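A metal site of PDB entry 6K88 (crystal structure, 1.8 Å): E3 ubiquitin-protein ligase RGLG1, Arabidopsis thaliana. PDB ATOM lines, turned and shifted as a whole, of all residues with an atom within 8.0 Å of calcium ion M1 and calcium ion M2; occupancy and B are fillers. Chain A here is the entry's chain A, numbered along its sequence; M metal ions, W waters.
The side-chain amide nitrogen of Gln 228 lies within hydrogen-bond range of the backbone carbonyl oxygen of Ser 252. The backbone NH of Gln 228 is in hydrogen-bond range of the backbone carbonyl oxygen of Ile 199. The backbone NH (N) of Phe 229 sits close to the side-chain carboxylate (OD2) of Asp 216 (3.2 Å). O of Asp 216 sits close to NH2 of Arg 222, 3.2 Å away. The side-chain carboxylate (OD1) of Asp 225 lies close to the guanidinium group (NH2) of Arg 222 (3.2 Å).
The side-chain carboxylate (OD1) of Asp 216 is bound to calcium ion M1 (2.3 Å). Calcium ion M1 is bound by OE1 of Glu 256 (2.3 Å). O of Asp 216 is bound to calcium ion M1, at 2.4 Å. OD1 of Asp 225 is bound to calcium ion M1, 2.4 Å away. The backbone carbonyl oxygen (O) of Phe 227 binds calcium ion M1 (2.4 Å). Water W2 binds calcium ion M1. The side-chain carboxylate (OD2) of Asp 225 binds calcium ion M1 (2.5 Å). The side-chain carboxylate (OE2) of Glu 256 is bound to calcium ion M1 (2.7 Å).
Three residues have an atom within 4 Å of calcium ion M2: Asp 216, Gln 228 and Glu 256.
Four residues have an atom within 4 Å of calcium ion M1: Asp 216, Asp 225, Phe 227 and Glu 256.
Calcium ion M2 is bound by OE1 of Gln 228 (2.3 Å), water W3 (2.3 Å), OE2 of Glu 256 (2.4 Å), water W1 (2.4 Å), water W4 (2.4 Å), OD2 of Asp 216 (2.5 Å) and OD1 of Asp 216 (2.6 Å). Calcium ion M2 has seven donor atoms within binding distance.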
ATOM      1  N   ILE A 199      -5.282  13.169  12.337  1.00  0.00           N
ATOM      2  CA  ILE A 199      -3.847  13.342  12.454  1.00  0.00           C
ATOM      3  C   ILE A 199      -3.316  14.100  11.246  1.00  0.00           C
ATOM      4  O   ILE A 199      -3.627  13.762  10.095  1.00  0.00           O
ATOM      5  CB  ILE A 199      -3.104  11.989  12.585  1.00  0.00           C
ATOM      6  CG1 ILE A 199      -3.685  11.177  13.727  1.00  0.00           C
ATOM      7  CG2 ILE A 199      -1.594  12.218  12.767  1.00  0.00           C
ATOM      8  CD1 ILE A 199      -3.269   9.701  13.701  1.00  0.00           C
ATOM      9  N   MET A 212       5.352   9.129   4.538  1.00  0.00           N
ATOM     10  CA  MET A 212       4.243   9.978   5.001  1.00  0.00           C
ATOM     11  C   MET A 212       3.097   9.907   4.010  1.00  0.00           C
ATOM     12  O   MET A 212       1.925   9.889   4.410  1.00  0.00           O
ATOM     13  CB  MET A 212       4.697  11.434   5.194  1.00  0.00           C
ATOM     14  CG  MET A 212       5.848  11.624   6.204  1.00  0.00           C
ATOM     15  SD  MET A 212       5.560  10.903   7.836  1.00  0.00           S
ATOM     16  CE  MET A 212       6.397   9.337   7.724  1.00  0.00           C
ATOM     17  N   GLN A 213       3.419   9.879   2.711  1.00  0.00           N
ATOM     18  CA  GLN A 213       2.390   9.807   1.678  1.00  0.00           C
ATOM     19  C   GLN A 213       1.647   8.472   1.774  1.00  0.00           C
ATOM     20  O   GLN A 213       0.444   8.390   1.518  1.00  0.00           O
ATOM     21  CB  GLN A 213       3.004   9.996   0.293  1.00  0.00           C
ATOM     22  CG  GLN A 213       3.270  11.460  -0.050  1.00  0.00           C
ATOM     23  CD  GLN A 213       4.315  11.643  -1.145  1.00  0.00           C
ATOM     24  OE1 GLN A 213       4.951  10.686  -1.579  1.00  0.00           O
ATOM     25  NE2 GLN A 213       4.502  12.888  -1.582  1.00  0.00           N
ATOM     26  N   GLU A 214       2.375   7.438   2.173  1.00  0.00           N
ATOM     27  CA  GLU A 214       1.760   6.145   2.418  1.00  0.00           C
ATOM     28  C   GLU A 214       0.842   6.155   3.641  1.00  0.00           C
ATOM     29  O   GLU A 214      -0.238   5.577   3.582  1.00  0.00           O
ATOM     30  CB  GLU A 214       2.844   5.072   2.597  1.00  0.00           C
ATOM     31  CG  GLU A 214       2.299   3.720   2.988  1.00  0.00           C
ATOM     32  CD  GLU A 214       2.805   2.601   2.100  1.00  0.00           C
ATOM     33  OE1 GLU A 214       2.903   2.806   0.865  1.00  0.00           O
ATOM     34  OE2 GLU A 214       3.109   1.509   2.636  1.00  0.00           O
ATOM     35  N   PHE A 215       1.260   6.796   4.740  1.00  0.00           N
ATOM     36  CA  PHE A 215       0.364   6.918   5.899  1.00  0.00           C
ATOM     37  C   PHE A 215      -0.877   7.734   5.520  1.00  0.00           C
ATOM     38  O   PHE A 215      -1.992   7.451   5.979  1.00  0.00           O
ATOM     39  CB  PHE A 215       1.065   7.565   7.113  1.00  0.00           C
ATOM     40  CG  PHE A 215       2.188   6.747   7.709  1.00  0.00           C
ATOM     41  CD1 PHE A 215       2.321   5.389   7.443  1.00  0.00           C
ATOM     42  CD2 PHE A 215       3.127   7.355   8.557  1.00  0.00           C
ATOM     43  CE1 PHE A 215       3.367   4.646   8.004  1.00  0.00           C
ATOM     44  CE2 PHE A 215       4.161   6.615   9.125  1.00  0.00           C
ATOM     45  CZ  PHE A 215       4.288   5.279   8.839  1.00  0.00           C
ATOM     46  N   ASP A 216      -0.660   8.747   4.677  1.00  0.00           N
ATOM     47  CA  ASP A 216      -1.719   9.626   4.198  1.00  0.00           C
ATOM     48  C   ASP A 216      -2.754   8.843   3.370  1.00  0.00           C
ATOM     49  O   ASP A 216      -3.957   8.958   3.601  1.00  0.00           O
ATOM     50  CB  ASP A 216      -1.110  10.762   3.352  1.00  0.00           C
ATOM     51  CG  ASP A 216      -2.118  11.851   2.964  1.00  0.00           C
ATOM     52  OD1 ASP A 216      -3.339  11.701   3.170  1.00  0.00           O
ATOM     53  OD2 ASP A 216      -1.671  12.886   2.427  1.00  0.00           O
ATOM     54  N   ASP A 217      -2.268   8.031   2.425  1.00  0.00           N
ATOM     55  CA  ASP A 217      -3.130   7.517   1.355  1.00  0.00           C
ATOM     56  C   ASP A 217      -3.421   6.022   1.406  1.00  0.00           C
ATOM     57  O   ASP A 217      -4.366   5.547   0.786  1.00  0.00           O
ATOM     58  CB  ASP A 217      -2.527   7.836  -0.016  1.00  0.00           C
ATOM     59  CG  ASP A 217      -2.372   9.335  -0.263  1.00  0.00           C
ATOM     60  OD1 ASP A 217      -3.214  10.137   0.208  1.00  0.00           O
ATOM     61  OD2 ASP A 217      -1.414   9.704  -0.973  1.00  0.00           O
ATOM     62  N   ASN A 218      -2.611   5.257   2.143  1.00  0.00           N
ATOM     63  CA  ASN A 218      -2.592   3.817   1.945  1.00  0.00           C
ATOM     64  C   ASN A 218      -2.451   2.977   3.213  1.00  0.00           C
ATOM     65  O   ASN A 218      -1.460   2.277   3.399  1.00  0.00           O
ATOM     66  CB  ASN A 218      -1.467   3.459   0.975  1.00  0.00           C
ATOM     67  CG  ASN A 218      -1.582   2.046   0.443  1.00  0.00           C
ATOM     68  OD1 ASN A 218      -2.654   1.439   0.469  1.00  0.00           O
ATOM     69  ND2 ASN A 218      -0.466   1.507  -0.033  1.00  0.00           N
ATOM     70  N   ARG A 222      -8.049   0.646   8.226  1.00  0.00           N
ATOM     71  CA  ARG A 222      -8.450   1.918   8.828  1.00  0.00           C
ATOM     72  C   ARG A 222      -9.968   2.166   8.789  1.00  0.00           C
ATOM     73  O   ARG A 222     -10.591   1.921   7.767  1.00  0.00           O
ATOM     74  CB  ARG A 222      -7.717   3.025   8.080  1.00  0.00           C
ATOM     75  CG  ARG A 222      -7.621   4.292   8.813  1.00  0.00           C
ATOM     76  CD  ARG A 222      -6.411   5.085   8.357  1.00  0.00           C
ATOM     77  NE  ARG A 222      -6.396   5.431   6.935  1.00  0.00           N
ATOM     78  CZ  ARG A 222      -5.467   6.221   6.411  1.00  0.00           C
ATOM     79  NH1 ARG A 222      -4.534   6.718   7.218  1.00  0.00           N
ATOM     80  NH2 ARG A 222      -5.456   6.514   5.118  1.00  0.00           N
ATOM     81  N   PHE A 224     -11.577   5.193   9.025  1.00  0.00           N
ATOM     82  CA  PHE A 224     -11.751   6.286   8.089  1.00  0.00           C
ATOM     83  C   PHE A 224     -10.372   6.873   7.795  1.00  0.00           C
ATOM     84  O   PHE A 224      -9.426   6.559   8.517  1.00  0.00           O
ATOM     85  CB  PHE A 224     -12.708   7.356   8.642  1.00  0.00           C
ATOM     86  CG  PHE A 224     -12.097   8.262   9.682  1.00  0.00           C
ATOM     87  CD1 PHE A 224     -11.886   7.817  10.973  1.00  0.00           C
ATOM     88  CD2 PHE A 224     -11.751   9.569   9.367  1.00  0.00           C
ATOM     89  CE1 PHE A 224     -11.329   8.659  11.944  1.00  0.00           C
ATOM     90  CE2 PHE A 224     -11.199  10.418  10.327  1.00  0.00           C
ATOM     91  CZ  PHE A 224     -10.992   9.966  11.614  1.00  0.00           C
ATOM     92  N   ASP A 225     -10.235   7.683   6.762  1.00  0.00           N
ATOM     93  CA  ASP A 225      -8.953   8.321   6.453  1.00  0.00           C
ATOM     94  C   ASP A 225      -8.619   9.371   7.516  1.00  0.00           C
ATOM     95  O   ASP A 225      -9.027  10.519   7.414  1.00  0.00           O
ATOM     96  CB  ASP A 225      -8.982   8.971   5.063  1.00  0.00           C
ATOM     97  CG  ASP A 225      -7.617   9.501   4.607  1.00  0.00           C
ATOM     98  OD1 ASP A 225      -6.649   9.481   5.396  1.00  0.00           O
ATOM     99  OD2 ASP A 225      -7.528   9.971   3.453  1.00  0.00           O
ATOM    100  N   ASN A 226      -7.853   8.961   8.529  1.00  0.00           N
ATOM    101  CA  ASN A 226      -7.551   9.850   9.673  1.00  0.00           C
ATOM    102  C   ASN A 226      -6.139  10.440   9.669  1.00  0.00           C
ATOM    103  O   ASN A 226      -5.684  10.966  10.690  1.00  0.00           O
ATOM    104  CB  ASN A 226      -7.746   9.082  10.979  1.00  0.00           C
ATOM    105  CG  ASN A 226      -6.743   7.940  11.132  1.00  0.00           C
ATOM    106  OD1 ASN A 226      -6.163   7.461  10.160  1.00  0.00           O
ATOM    107  ND2 ASN A 226      -6.543   7.513  12.367  1.00  0.00           N
ATOM    108  N   PHE A 227      -5.447  10.345   8.534  1.00  0.00           N
ATOM    109  CA  PHE A 227      -4.075  10.831   8.456  1.00  0.00           C
ATOM    110  C   PHE A 227      -3.888  11.695   7.213  1.00  0.00           C
ATOM    111  O   PHE A 227      -4.113  11.234   6.090  1.00  0.00           O
ATOM    112  CB  PHE A 227      -3.107   9.651   8.432  1.00  0.00           C
ATOM    113  CG  PHE A 227      -1.668  10.020   8.695  1.00  0.00           C
ATOM    114  CD1 PHE A 227      -0.906  10.673   7.731  1.00  0.00           C
ATOM    115  CD2 PHE A 227      -1.059   9.666   9.890  1.00  0.00           C
ATOM    116  CE1 PHE A 227       0.424  10.979   7.958  1.00  0.00           C
ATOM    117  CE2 PHE A 227       0.279   9.974  10.132  1.00  0.00           C
ATOM    118  CZ  PHE A 227       1.016  10.647   9.173  1.00  0.00           C
ATOM    119  N   GLN A 228      -3.488  12.945   7.424  1.00  0.00           N
ATOM    120  CA  GLN A 228      -3.186  13.875   6.342  1.00  0.00           C
ATOM    121  C   GLN A 228      -1.714  14.289   6.353  1.00  0.00           C
ATOM    122  O   GLN A 228      -1.148  14.577   7.418  1.00  0.00           O
ATOM    123  CB  GLN A 228      -4.091  15.108   6.425  1.00  0.00           C
ATOM    124  CG  GLN A 228      -3.630  16.338   5.631  1.00  0.00           C
ATOM    125  CD  GLN A 228      -3.840  16.183   4.134  1.00  0.00           C
ATOM    126  OE1 GLN A 228      -3.719  15.088   3.594  1.00  0.00           O
ATOM    127  NE2 GLN A 228      -4.165  17.281   3.469  1.00  0.00           N
ATOM    128  N   PHE A 229      -1.084  14.296   5.184  1.00  0.00           N
ATOM    129  CA  PHE A 229       0.275  14.815   5.043  1.00  0.00           C
ATOM    130  C   PHE A 229       0.280  16.202   4.391  1.00  0.00           C
ATOM    131  O   PHE A 229      -0.297  16.381   3.322  1.00  0.00           O
ATOM    132  CB  PHE A 229       1.153  13.842   4.238  1.00  0.00           C
ATOM    133  CG  PHE A 229       2.464  14.428   3.797  1.00  0.00           C
ATOM    134  CD1 PHE A 229       3.410  14.804   4.735  1.00  0.00           C
ATOM    135  CD2 PHE A 229       2.753  14.610   2.456  1.00  0.00           C
ATOM    136  CE1 PHE A 229       4.626  15.369   4.339  1.00  0.00           C
ATOM    137  CE2 PHE A 229       3.965  15.166   2.056  1.00  0.00           C
ATOM    138  CZ  PHE A 229       4.895  15.536   2.998  1.00  0.00           C
ATOM    139  N   VAL A 230       0.910  17.174   5.057  1.00  0.00           N
ATOM    140  CA  VAL A 230       1.161  18.479   4.461  1.00  0.00           C
ATOM    141  C   VAL A 230       2.651  18.755   4.414  1.00  0.00           C
ATOM    142  O   VAL A 230       3.337  18.705   5.447  1.00  0.00           O
ATOM    143  CB  VAL A 230       0.487  19.611   5.252  1.00  0.00           C
ATOM    144  CG1 VAL A 230       0.750  20.965   4.585  1.00  0.00           C
ATOM    145  CG2 VAL A 230      -1.005  19.358   5.359  1.00  0.00           C
ATOM    146  N   SER A 252      -4.850  23.084   3.723  1.00  0.00           N
ATOM    147  CA  SER A 252      -4.315  21.750   3.425  1.00  0.00           C
ATOM    148  C   SER A 252      -4.347  20.886   4.663  1.00  0.00           C
ATOM    149  O   SER A 252      -4.743  19.734   4.609  1.00  0.00           O
ATOM    150  CB  SER A 252      -2.882  21.832   2.891  1.00  0.00           C
ATOM    151  OG  SER A 252      -2.860  22.414   1.604  1.00  0.00           O
ATOM    152  N   MET A 255      -7.848  19.775   5.234  1.00  0.00           N
ATOM    153  CA  MET A 255      -8.516  19.272   4.034  1.00  0.00           C
ATOM    154  C   MET A 255      -9.278  17.962   4.260  1.00  0.00           C
ATOM    155  O   MET A 255     -10.360  17.777   3.720  1.00  0.00           O
ATOM    156  CB  MET A 255      -7.494  19.098   2.913  1.00  0.00           C
ATOM    157  CG  MET A 255      -8.076  18.660   1.576  1.00  0.00           C
ATOM    158  SD  MET A 255      -9.134  19.933   0.837  1.00  0.00           S
ATOM    159  CE  MET A 255      -7.967  21.292   0.717  1.00  0.00           C
ATOM    160  N   GLU A 256      -8.727  17.073   5.075  1.00  0.00           N
ATOM    161  CA  GLU A 256      -9.326  15.758   5.298  1.00  0.00           C
ATOM    162  C   GLU A 256     -10.110  15.626   6.597  1.00  0.00           C
ATOM    163  O   GLU A 256     -10.432  14.509   7.021  1.00  0.00           O
ATOM    164  CB  GLU A 256      -8.243  14.675   5.277  1.00  0.00           C
ATOM    165  CG  GLU A 256      -7.424  14.658   4.012  1.00  0.00           C
ATOM    166  CD  GLU A 256      -6.515  13.450   3.925  1.00  0.00           C
ATOM    167  OE1 GLU A 256      -6.467  12.668   4.906  1.00  0.00           O
ATOM    168  OE2 GLU A 256      -5.866  13.263   2.884  1.00  0.00           O
HETATM  169 CA    CA M   1      -5.288  10.879   3.986  1.00  0.00          CA
HETATM  170 CA    CA M   2      -3.859  13.777   1.754  1.00  0.00          CA
HETATM  171  O   HOH W   1      -3.394  12.705  -0.373  1.00  0.00           O
HETATM  172  O   HOH W   2      -5.551  10.469   1.581  1.00  0.00           O
HETATM  173  O   HOH W   3      -2.384  15.347   1.014  1.00  0.00           O
HETATM  174  O   HOH W   4      -5.292  15.266   0.476  1.00  0.00           O
